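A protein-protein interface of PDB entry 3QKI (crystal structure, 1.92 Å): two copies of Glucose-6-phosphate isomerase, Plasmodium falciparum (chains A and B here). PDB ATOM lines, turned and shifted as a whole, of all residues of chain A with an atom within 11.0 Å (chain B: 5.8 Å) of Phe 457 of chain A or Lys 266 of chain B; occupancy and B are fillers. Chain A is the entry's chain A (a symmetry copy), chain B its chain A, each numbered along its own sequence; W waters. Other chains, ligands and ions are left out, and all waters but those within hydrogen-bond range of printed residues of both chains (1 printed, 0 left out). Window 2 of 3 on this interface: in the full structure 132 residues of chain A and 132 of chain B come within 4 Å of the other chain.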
ATOM      1  N   GLN A 204     -12.670 -21.220  -9.855  1.00  0.00           N
ATOM      2  CA  GLN A 204     -13.347 -21.654  -8.631  1.00  0.00           C
ATOM      3  C   GLN A 204     -13.339 -20.608  -7.520  1.00  0.00           C
ATOM      4  O   GLN A 204     -12.362 -19.881  -7.349  1.00  0.00           O
ATOM      5  CB  GLN A 204     -12.781 -22.988  -8.136  1.00  0.00           C
ATOM      6  N   VAL A 205     -14.450 -20.547  -6.768  1.00  0.00           N
ATOM      7  CA  VAL A 205     -14.703 -19.622  -5.661  1.00  0.00           C
ATOM      8  C   VAL A 205     -15.053 -20.453  -4.430  1.00  0.00           C
ATOM      9  O   VAL A 205     -15.242 -21.671  -4.550  1.00  0.00           O
ATOM     10  CB  VAL A 205     -15.859 -18.621  -5.998  1.00  0.00           C
ATOM     11  CG1 VAL A 205     -15.484 -17.691  -7.140  1.00  0.00           C
ATOM     12  CG2 VAL A 205     -17.167 -19.342  -6.299  1.00  0.00           C
ATOM     13  N   ASN A 206     -15.171 -19.794  -3.257  1.00  0.00           N
ATOM     14  CA  ASN A 206     -15.629 -20.390  -2.019  1.00  0.00           C
ATOM     15  C   ASN A 206     -14.826 -21.613  -1.576  1.00  0.00           C
ATOM     16  O   ASN A 206     -15.407 -22.640  -1.222  1.00  0.00           O
ATOM     17  CB  ASN A 206     -17.175 -20.686  -2.102  1.00  0.00           C
ATOM     18  CG  ASN A 206     -18.006 -19.530  -2.625  1.00  0.00           C
ATOM     19  OD1 ASN A 206     -17.565 -18.377  -2.668  1.00  0.00           O
ATOM     20  ND2 ASN A 206     -19.245 -19.792  -3.008  1.00  0.00           N
ATOM     21  N   ASN A 207     -13.486 -21.482  -1.547  1.00  0.00           N
ATOM     22  CA  ASN A 207     -12.604 -22.571  -1.153  1.00  0.00           C
ATOM     23  C   ASN A 207     -12.547 -22.790   0.362  1.00  0.00           C
ATOM     24  O   ASN A 207     -11.471 -22.905   0.943  1.00  0.00           O
ATOM     25  CB  ASN A 207     -11.223 -22.399  -1.783  1.00  0.00           C
ATOM     26  CG  ASN A 207     -11.279 -22.187  -3.273  1.00  0.00           C
ATOM     27  OD1 ASN A 207     -11.157 -21.063  -3.773  1.00  0.00           O
ATOM     28  ND2 ASN A 207     -11.525 -23.242  -4.015  1.00  0.00           N
ATOM     29  N   PHE A 208     -13.720 -22.909   0.995  1.00  0.00           N
ATOM     30  CA  PHE A 208     -13.827 -23.079   2.449  1.00  0.00           C
ATOM     31  C   PHE A 208     -13.267 -24.380   3.007  1.00  0.00           C
ATOM     32  O   PHE A 208     -13.005 -24.450   4.202  1.00  0.00           O
ATOM     33  CB  PHE A 208     -15.277 -22.855   2.925  1.00  0.00           C
ATOM     34  CG  PHE A 208     -15.793 -21.463   2.686  1.00  0.00           C
ATOM     35  CD1 PHE A 208     -15.382 -20.411   3.487  1.00  0.00           C
ATOM     36  CD2 PHE A 208     -16.711 -21.210   1.673  1.00  0.00           C
ATOM     37  CE1 PHE A 208     -15.862 -19.124   3.272  1.00  0.00           C
ATOM     38  CE2 PHE A 208     -17.202 -19.922   1.469  1.00  0.00           C
ATOM     39  CZ  PHE A 208     -16.768 -18.885   2.267  1.00  0.00           C
ATOM     40  N   ASN A 209     -13.071 -25.395   2.154  1.00  0.00           N
ATOM     41  CA  ASN A 209     -12.509 -26.664   2.592  1.00  0.00           C
ATOM     42  C   ASN A 209     -10.974 -26.698   2.523  1.00  0.00           C
ATOM     43  O   ASN A 209     -10.380 -27.758   2.755  1.00  0.00           O
ATOM     44  CB  ASN A 209     -13.131 -27.839   1.830  1.00  0.00           C
ATOM     45  CG  ASN A 209     -14.529 -28.189   2.290  1.00  0.00           C
ATOM     46  OD1 ASN A 209     -14.941 -27.932   3.447  1.00  0.00           O
ATOM     47  ND2 ASN A 209     -15.288 -28.799   1.383  1.00  0.00           N
ATOM     48  N   PHE A 453      -8.569 -15.350  -2.082  1.00  0.00           N
ATOM     49  CA  PHE A 453      -9.649 -16.199  -1.575  1.00  0.00           C
ATOM     50  C   PHE A 453     -10.993 -15.743  -2.181  1.00  0.00           C
ATOM     51  O   PHE A 453     -11.800 -15.155  -1.479  1.00  0.00           O
ATOM     52  CB  PHE A 453      -9.669 -16.190  -0.034  1.00  0.00           C
ATOM     53  CG  PHE A 453     -10.476 -17.312   0.585  1.00  0.00           C
ATOM     54  CD1 PHE A 453     -10.004 -18.620   0.573  1.00  0.00           C
ATOM     55  CD2 PHE A 453     -11.706 -17.054   1.199  1.00  0.00           C
ATOM     56  CE1 PHE A 453     -10.749 -19.651   1.159  1.00  0.00           C
ATOM     57  CE2 PHE A 453     -12.447 -18.087   1.782  1.00  0.00           C
ATOM     58  CZ  PHE A 453     -11.969 -19.375   1.748  1.00  0.00           C
ATOM     59  N   PRO A 454     -11.233 -15.965  -3.493  1.00  0.00           N
ATOM     60  CA  PRO A 454     -12.481 -15.464  -4.096  1.00  0.00           C
ATOM     61  C   PRO A 454     -13.734 -16.091  -3.487  1.00  0.00           C
ATOM     62  O   PRO A 454     -13.798 -17.286  -3.210  1.00  0.00           O
ATOM     63  CB  PRO A 454     -12.328 -15.788  -5.586  1.00  0.00           C
ATOM     64  CG  PRO A 454     -11.293 -16.813  -5.666  1.00  0.00           C
ATOM     65  CD  PRO A 454     -10.392 -16.655  -4.495  1.00  0.00           C
ATOM     66  N   ILE A 455     -14.684 -15.242  -3.192  1.00  0.00           N
ATOM     67  CA  ILE A 455     -15.978 -15.602  -2.648  1.00  0.00           C
ATOM     68  C   ILE A 455     -17.040 -15.004  -3.539  1.00  0.00           C
ATOM     69  O   ILE A 455     -16.975 -13.817  -3.877  1.00  0.00           O
ATOM     70  CB  ILE A 455     -16.163 -15.165  -1.160  1.00  0.00           C
ATOM     71  CG1 ILE A 455     -15.166 -15.890  -0.226  1.00  0.00           C
ATOM     72  CG2 ILE A 455     -17.615 -15.400  -0.719  1.00  0.00           C
ATOM     73  CD1 ILE A 455     -15.165 -15.401   1.193  1.00  0.00           C
ATOM     74  N   LYS A 456     -18.068 -15.808  -3.830  1.00  0.00           N
ATOM     75  CA  LYS A 456     -19.229 -15.390  -4.607  1.00  0.00           C
ATOM     76  C   LYS A 456     -20.379 -16.340  -4.369  1.00  0.00           C
ATOM     77  O   LYS A 456     -20.247 -17.557  -4.570  1.00  0.00           O
ATOM     78  CB  LYS A 456     -18.891 -15.309  -6.103  1.00  0.00           C
ATOM     79  CG  LYS A 456     -20.040 -14.841  -6.986  1.00  0.00           C
ATOM     80  CD  LYS A 456     -19.551 -14.186  -8.281  1.00  0.00           C
ATOM     81  CE  LYS A 456     -18.933 -15.145  -9.286  1.00  0.00           C
ATOM     82  NZ  LYS A 456     -17.464 -15.288  -9.106  1.00  0.00           N
ATOM     83  N   PHE A 457     -21.506 -15.779  -3.941  1.00  0.00           N
ATOM     84  CA  PHE A 457     -22.739 -16.530  -3.742  1.00  0.00           C
ATOM     85  C   PHE A 457     -23.744 -16.093  -4.810  1.00  0.00           C
ATOM     86  O   PHE A 457     -23.799 -14.898  -5.157  1.00  0.00           O
ATOM     87  CB  PHE A 457     -23.274 -16.381  -2.317  1.00  0.00           C
ATOM     88  CG  PHE A 457     -22.264 -16.787  -1.268  1.00  0.00           C
ATOM     89  CD1 PHE A 457     -21.627 -15.825  -0.481  1.00  0.00           C
ATOM     90  CD2 PHE A 457     -21.918 -18.126  -1.089  1.00  0.00           C
ATOM     91  CE1 PHE A 457     -20.693 -16.193   0.476  1.00  0.00           C
ATOM     92  CE2 PHE A 457     -20.965 -18.495  -0.127  1.00  0.00           C
ATOM     93  CZ  PHE A 457     -20.360 -17.526   0.648  1.00  0.00           C
ATOM     94  N   ASP A 458     -24.499 -17.088  -5.342  1.00  0.00           N
ATOM     95  CA  ASP A 458     -25.463 -16.914  -6.438  1.00  0.00           C
ATOM     96  C   ASP A 458     -26.370 -15.689  -6.370  1.00  0.00           C
ATOM     97  O   ASP A 458     -26.451 -14.964  -7.365  1.00  0.00           O
ATOM     98  CB  ASP A 458     -26.276 -18.195  -6.716  1.00  0.00           C
ATOM     99  CG  ASP A 458     -25.475 -19.370  -7.244  1.00  0.00           C
ATOM    100  OD1 ASP A 458     -24.457 -19.138  -7.943  1.00  0.00           O
ATOM    101  OD2 ASP A 458     -25.890 -20.519  -7.000  1.00  0.00           O
ATOM    102  N   LYS A 459     -27.017 -15.443  -5.230  1.00  0.00           N
ATOM    103  CA  LYS A 459     -27.939 -14.332  -5.021  1.00  0.00           C
ATOM    104  C   LYS A 459     -27.306 -12.956  -4.853  1.00  0.00           C
ATOM    105  O   LYS A 459     -28.017 -11.953  -4.946  1.00  0.00           O
ATOM    106  CB  LYS A 459     -28.870 -14.653  -3.825  1.00  0.00           C
ATOM    107  N   GLU A 460     -25.984 -12.896  -4.612  1.00  0.00           N
ATOM    108  CA  GLU A 460     -25.302 -11.618  -4.411  1.00  0.00           C
ATOM    109  C   GLU A 460     -25.190 -10.817  -5.678  1.00  0.00           C
ATOM    110  O   GLU A 460     -24.994 -11.384  -6.749  1.00  0.00           O
ATOM    111  CB  GLU A 460     -23.904 -11.832  -3.804  1.00  0.00           C
ATOM    112  CG  GLU A 460     -23.937 -12.451  -2.415  1.00  0.00           C
ATOM    113  CD  GLU A 460     -24.493 -11.576  -1.307  1.00  0.00           C
ATOM    114  OE1 GLU A 460     -24.516 -10.330  -1.455  1.00  0.00           O
ATOM    115  OE2 GLU A 460     -24.877 -12.154  -0.266  1.00  0.00           O
ATOM    116  N   VAL A 461     -25.294  -9.489  -5.554  1.00  0.00           N
ATOM    117  CA  VAL A 461     -25.158  -8.555  -6.691  1.00  0.00           C
ATOM    118  C   VAL A 461     -23.752  -8.687  -7.308  1.00  0.00           C
ATOM    119  O   VAL A 461     -23.610  -8.766  -8.531  1.00  0.00           O
ATOM    120  CB  VAL A 461     -25.490  -7.103  -6.214  1.00  0.00           C
ATOM    121  CG1 VAL A 461     -25.079  -6.058  -7.251  1.00  0.00           C
ATOM    122  CG2 VAL A 461     -26.978  -6.961  -5.873  1.00  0.00           C
ATOM    123  N   VAL A 462     -22.720  -8.769  -6.456  1.00  0.00           N
ATOM    124  CA  VAL A 462     -21.327  -8.922  -6.901  1.00  0.00           C
ATOM    125  C   VAL A 462     -20.549  -9.912  -6.037  1.00  0.00           C
ATOM    126  O   VAL A 462     -20.927 -10.181  -4.890  1.00  0.00           O
ATOM    127  CB  VAL A 462     -20.580  -7.550  -6.947  1.00  0.00           C
ATOM    128  CG1 VAL A 462     -21.021  -6.691  -8.125  1.00  0.00           C
ATOM    129  CG2 VAL A 462     -20.696  -6.789  -5.626  1.00  0.00           C
ATOM    130  N   SER A 463     -19.401 -10.371  -6.547  1.00  0.00           N
ATOM    131  CA  SER A 463     -18.458 -11.178  -5.776  1.00  0.00           C
ATOM    132  C   SER A 463     -17.919 -10.239  -4.680  1.00  0.00           C
ATOM    133  O   SER A 463     -17.933  -9.005  -4.855  1.00  0.00           O
ATOM    134  CB  SER A 463     -17.308 -11.646  -6.663  1.00  0.00           C
ATOM    135  OG  SER A 463     -16.431 -10.592  -7.021  1.00  0.00           O
ATOM    136  N   ASN A 464     -17.460 -10.798  -3.564  1.00  0.00           N
ATOM    137  CA  ASN A 464     -16.924 -10.003  -2.465  1.00  0.00           C
ATOM    138  C   ASN A 464     -15.739  -9.146  -2.915  1.00  0.00           C
ATOM    139  O   ASN A 464     -15.615  -8.006  -2.492  1.00  0.00           O
ATOM    140  CB  ASN A 464     -16.564 -10.912  -1.278  1.00  0.00           C
ATOM    141  CG  ASN A 464     -17.727 -11.721  -0.744  1.00  0.00           C
ATOM    142  OD1 ASN A 464     -18.596 -12.159  -1.496  1.00  0.00           O
ATOM    143  ND2 ASN A 464     -17.745 -11.983   0.565  1.00  0.00           N
ATOM    144  N   HIS A 465     -14.892  -9.682  -3.820  1.00  0.00           N
ATOM    145  CA  HIS A 465     -13.719  -8.960  -4.320  1.00  0.00           C
ATOM    146  C   HIS A 465     -14.168  -7.764  -5.162  1.00  0.00           C
ATOM    147  O   HIS A 465     -13.581  -6.686  -5.040  1.00  0.00           O
ATOM    148  CB  HIS A 465     -12.759  -9.885  -5.098  1.00  0.00           C
ATOM    149  CG  HIS A 465     -11.487  -9.192  -5.490  1.00  0.00           C
ATOM    150  ND1 HIS A 465     -10.498  -8.913  -4.565  1.00  0.00           N
ATOM    151  CD2 HIS A 465     -11.131  -8.661  -6.681  1.00  0.00           C
ATOM    152  CE1 HIS A 465      -9.564  -8.258  -5.236  1.00  0.00           C
ATOM    153  NE2 HIS A 465      -9.908  -8.079  -6.510  1.00  0.00           N
ATOM    154  N   ASP A 466     -15.239  -7.939  -5.979  1.00  0.00           N
ATOM    155  CA  ASP A 466     -15.812  -6.823  -6.752  1.00  0.00           C
ATOM    156  C   ASP A 466     -16.388  -5.787  -5.799  1.00  0.00           C
ATOM    157  O   ASP A 466     -16.193  -4.603  -6.041  1.00  0.00           O
ATOM    158  CB  ASP A 466     -16.884  -7.296  -7.736  1.00  0.00           C
ATOM    159  CG  ASP A 466     -16.350  -7.729  -9.082  1.00  0.00           C
ATOM    160  OD1 ASP A 466     -15.102  -7.747  -9.257  1.00  0.00           O
ATOM    161  OD2 ASP A 466     -17.170  -8.063  -9.956  1.00  0.00           O
ATOM    162  N   GLU A 467     -17.034  -6.214  -4.701  1.00  0.00           N
ATOM    163  CA  GLU A 467     -17.566  -5.268  -3.708  1.00  0.00           C
ATOM    164  C   GLU A 467     -16.428  -4.392  -3.129  1.00  0.00           C
ATOM    165  O   GLU A 467     -16.577  -3.176  -3.067  1.00  0.00           O
ATOM    166  CB  GLU A 467     -18.370  -5.980  -2.593  1.00  0.00           C
ATOM    167  CG  GLU A 467     -18.931  -5.033  -1.527  1.00  0.00           C
ATOM    168  CD  GLU A 467     -19.965  -4.026  -2.010  1.00  0.00           C
ATOM    169  OE1 GLU A 467     -20.660  -4.324  -3.003  1.00  0.00           O
ATOM    170  OE2 GLU A 467     -20.100  -2.953  -1.384  1.00  0.00           O
ATOM    171  N   LEU B 259     -22.472  -8.227   4.116  1.00  0.00           N
ATOM    172  CA  LEU B 259     -21.944  -9.194   3.141  1.00  0.00           C
ATOM    173  C   LEU B 259     -21.034 -10.202   3.889  1.00  0.00           C
ATOM    174  O   LEU B 259     -21.083 -11.405   3.606  1.00  0.00           O
ATOM    175  CB  LEU B 259     -21.184  -8.493   1.994  1.00  0.00           C
ATOM    176  CG  LEU B 259     -20.473  -9.386   0.956  1.00  0.00           C
ATOM    177  CD1 LEU B 259     -21.466 -10.433   0.316  1.00  0.00           C
ATOM    178  CD2 LEU B 259     -19.800  -8.532  -0.116  1.00  0.00           C
ATOM    179  N   ALA B 261     -21.331 -10.979   7.124  1.00  0.00           N
ATOM    180  CA  ALA B 261     -22.257 -11.764   7.942  1.00  0.00           C
ATOM    181  C   ALA B 261     -22.889 -12.889   7.108  1.00  0.00           C
ATOM    182  O   ALA B 261     -22.891 -14.045   7.538  1.00  0.00           O
ATOM    183  CB  ALA B 261     -23.339 -10.862   8.543  1.00  0.00           C
ATOM    184  N   ARG B 262     -23.363 -12.572   5.897  1.00  0.00           N
ATOM    185  CA  ARG B 262     -23.943 -13.583   5.002  1.00  0.00           C
ATOM    186  C   ARG B 262     -22.905 -14.643   4.624  1.00  0.00           C
ATOM    187  O   ARG B 262     -23.225 -15.844   4.618  1.00  0.00           O
ATOM    188  CB  ARG B 262     -24.575 -12.953   3.748  1.00  0.00           C
ATOM    189  CG  ARG B 262     -25.834 -12.143   4.066  1.00  0.00           C
ATOM    190  CD  ARG B 262     -26.533 -11.648   2.812  1.00  0.00           C
ATOM    191  NE  ARG B 262     -25.700 -10.813   1.930  1.00  0.00           N
ATOM    192  CZ  ARG B 262     -25.573  -9.493   2.047  1.00  0.00           C
ATOM    193  NH1 ARG B 262     -26.179  -8.842   3.032  1.00  0.00           N
ATOM    194  NH2 ARG B 262     -24.839  -8.815   1.181  1.00  0.00           N
ATOM    195  N   SER B 263     -21.648 -14.210   4.396  1.00  0.00           N
ATOM    196  CA  SER B 263     -20.548 -15.107   4.061  1.00  0.00           C
ATOM    197  C   SER B 263     -20.208 -16.043   5.228  1.00  0.00           C
ATOM    198  O   SER B 263     -20.013 -17.239   5.019  1.00  0.00           O
ATOM    199  CB  SER B 263     -19.327 -14.301   3.612  1.00  0.00           C
ATOM    200  OG  SER B 263     -19.633 -13.474   2.497  1.00  0.00           O
ATOM    201  N   ILE B 264     -20.177 -15.505   6.454  1.00  0.00           N
ATOM    202  CA  ILE B 264     -19.873 -16.298   7.644  1.00  0.00           C
ATOM    203  C   ILE B 264     -21.033 -17.235   8.003  1.00  0.00           C
ATOM    204  O   ILE B 264     -20.786 -18.348   8.481  1.00  0.00           O
ATOM    205  CB  ILE B 264     -19.314 -15.450   8.818  1.00  0.00           C
ATOM    206  CG1 ILE B 264     -17.922 -14.869   8.444  1.00  0.00           C
ATOM    207  CG2 ILE B 264     -19.255 -16.229  10.158  1.00  0.00           C
ATOM    208  CD1 ILE B 264     -16.765 -15.928   8.207  1.00  0.00           C
ATOM    209  N   LYS B 265     -22.272 -16.815   7.719  1.00  0.00           N
ATOM    210  CA  LYS B 265     -23.448 -17.658   7.936  1.00  0.00           C
ATOM    211  C   LYS B 265     -23.381 -18.856   6.952  1.00  0.00           C
ATOM    212  O   LYS B 265     -23.681 -19.972   7.356  1.00  0.00           O
ATOM    213  CB  LYS B 265     -24.745 -16.866   7.743  1.00  0.00           C
ATOM    214  CG  LYS B 265     -26.004 -17.665   8.067  1.00  0.00           C
ATOM    215  CD  LYS B 265     -27.228 -16.821   7.758  1.00  0.00           C
ATOM    216  CE  LYS B 265     -28.489 -17.467   8.237  1.00  0.00           C
ATOM    217  NZ  LYS B 265     -29.678 -16.764   7.686  1.00  0.00           N
ATOM    218  N   LYS B 266     -22.944 -18.620   5.687  1.00  0.00           N
ATOM    219  CA  LYS B 266     -22.743 -19.675   4.694  1.00  0.00           C
ATOM    220  C   LYS B 266     -21.652 -20.643   5.195  1.00  0.00           C
ATOM    221  O   LYS B 266     -21.847 -21.851   5.109  1.00  0.00           O
ATOM    222  CB  LYS B 266     -22.335 -19.093   3.326  1.00  0.00           C
ATOM    223  CG  LYS B 266     -23.475 -18.419   2.573  1.00  0.00           C
ATOM    224  CD  LYS B 266     -24.205 -19.367   1.663  1.00  0.00           C
ATOM    225  CE  LYS B 266     -25.515 -18.777   1.174  1.00  0.00           C
ATOM    226  NZ  LYS B 266     -25.312 -17.732   0.134  1.00  0.00           N
ATOM    227  N   TRP B 267     -20.537 -20.117   5.760  1.00  0.00           N
ATOM    228  CA  TRP B 267     -19.451 -20.935   6.318  1.00  0.00           C
ATOM    229  C   TRP B 267     -19.977 -21.774   7.508  1.00  0.00           C
ATOM    230  O   TRP B 267     -19.702 -22.980   7.562  1.00  0.00           O
ATOM    231  CB  TRP B 267     -18.263 -20.054   6.738  1.00  0.00           C
ATOM    232  CG  TRP B 267     -17.187 -20.769   7.515  1.00  0.00           C
ATOM    233  CD1 TRP B 267     -16.233 -21.615   7.015  1.00  0.00           C
ATOM    234  CD2 TRP B 267     -16.961 -20.698   8.928  1.00  0.00           C
ATOM    235  NE1 TRP B 267     -15.437 -22.085   8.029  1.00  0.00           N
ATOM    236  CE2 TRP B 267     -15.841 -21.516   9.214  1.00  0.00           C
ATOM    237  CE3 TRP B 267     -17.619 -20.047   9.991  1.00  0.00           C
ATOM    238  CZ2 TRP B 267     -15.315 -21.640  10.503  1.00  0.00           C
ATOM    239  CZ3 TRP B 267     -17.096 -20.173  11.276  1.00  0.00           C
ATOM    240  CH2 TRP B 267     -15.965 -20.971  11.524  1.00  0.00           C
ATOM    241  N   LEU B 268     -20.745 -21.142   8.440  1.00  0.00           N
ATOM    242  CA  LEU B 268     -21.338 -21.883   9.570  1.00  0.00           C
ATOM    243  C   LEU B 268     -22.242 -23.026   9.047  1.00  0.00           C
ATOM    244  O   LEU B 268     -22.186 -24.136   9.580  1.00  0.00           O
ATOM    245  CB  LEU B 268     -22.196 -20.978  10.491  1.00  0.00           C
ATOM    246  CG  LEU B 268     -21.504 -20.020  11.461  1.00  0.00           C
ATOM    247  CD1 LEU B 268     -22.573 -19.220  12.233  1.00  0.00           C
ATOM    248  CD2 LEU B 268     -20.589 -20.765  12.454  1.00  0.00           C
ATOM    249  N   SER B 269     -23.049 -22.747   8.000  1.00  0.00           N
ATOM    250  CA  SER B 269     -24.019 -23.678   7.405  1.00  0.00           C
ATOM    251  C   SER B 269     -23.412 -24.849   6.632  1.00  0.00           C
ATOM    252  O   SER B 269     -24.138 -25.744   6.218  1.00  0.00           O
ATOM    253  CB  SER B 269     -25.035 -22.936   6.544  1.00  0.00           C
ATOM    254  OG  SER B 269     -25.740 -22.013   7.354  1.00  0.00           O
ATOM    255  N   LEU B 270     -22.099 -24.856   6.447  1.00  0.00           N
ATOM    256  CA  LEU B 270     -21.410 -25.981   5.827  1.00  0.00           C
ATOM    257  C   LEU B 270     -21.481 -27.175   6.799  1.00  0.00           C
ATOM    258  O   LEU B 270     -21.500 -28.321   6.357  1.00  0.00           O
ATOM    259  CB  LEU B 270     -19.936 -25.631   5.519  1.00  0.00           C
ATOM    260  CG  LEU B 270     -19.708 -24.549   4.448  1.00  0.00           C
ATOM    261  CD1 LEU B 270     -18.265 -24.164   4.380  1.00  0.00           C
ATOM    262  CD2 LEU B 270     -20.165 -24.993   3.067  1.00  0.00           C
HETATM  263  O   HOH W   1     -13.960 -24.043   6.638  1.00  0.00           O
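The side-chain amide nitrogen (ND2) of Asn 464 of chain A lies within hydrogen-bond range of the side-chain hydroxyl (OG) of Ser 263 of chain B (3.1 Å).
The guanidinium group of Arg 262 of chain B is in salt-bridge range of the side-chain carboxylate of Glu 460 of chain A, 2.7 Å away.
N of Asn 464 of chain A lies within hydrogen-bond range of O of Ile 455 of chain A.
The backbone carbonyl oxygen (O) of Leu 259 of chain B lies within hydrogen-bond range of the side-chain hydroxyl (OG) of Ser 263 of chain B (2.8 Å).
Among the printed residues, pairs that only touch across the chains: Phe 457 of chain A with Lys 266 of chain B (3.5 Å), Glu 460 of chain A with Leu 259 of chain B (3.5 Å), Phe 457 of chain A with Ser 263 of chain B (3.5 Å), Phe 208 of chain A with Leu 270 of chain B (3.6 Å), Asn 464 of chain A with Leu 259 of chain B (3.8 Å), Phe 208 of chain A with Trp 267 of chain B (3.8 Å) and Glu 467 of chain A with Leu 259 of chain B (3.8 Å).
Of the printed residues of chain B, Phe 208 of chain A touches Trp 267 (3.8 Å) and Leu 270 (3.6 Å).
Of chain B, only Ser 263 (3.5 Å) and Lys 266 (3.5 Å) come within 4 Å of Phe 457 of chain A.
Printed residues of chain B within 4 Å of Glu 467 of chain A: Leu 259 (3.8 Å).
Of chain A, only Phe 457 and Asn 464 come within 4 Å of Ser 263 of chain B.
No residue of chain A comes within 4 Å of Ser 269 of chain B.
Of chain A, only Phe 208 (3.6 Å) comes within 4 Å of Leu 270 of chain B.
Printed residues of chain B that touch a printed residue of chain A: Leu 259, Arg 262, Ser 263, Lys 266, Trp 267 and Leu 270.
Of the 21 printed residues of chain A, 5 touch a printed residue of chain B.
Hydrophobic or aromatic side chains of chain A within 4 Å of the printed part of chain B: Phe 208 and Phe 457.
Among the printed residues, Asp or Glu carboxylates within 4 Å of a Lys or Arg side-chain nitrogen of the other chain: Glu 460 of chain A with Arg 262 of chain B (2.7 Å).
No position is printed for both chains.
Water W1 lies within hydrogen-bond range of the backbone carbonyl oxygen (O) of Phe 208 of chain A (2.6 Å) and the indole nitrogen (NE1) of Trp 267 of chain B (2.8 Å).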
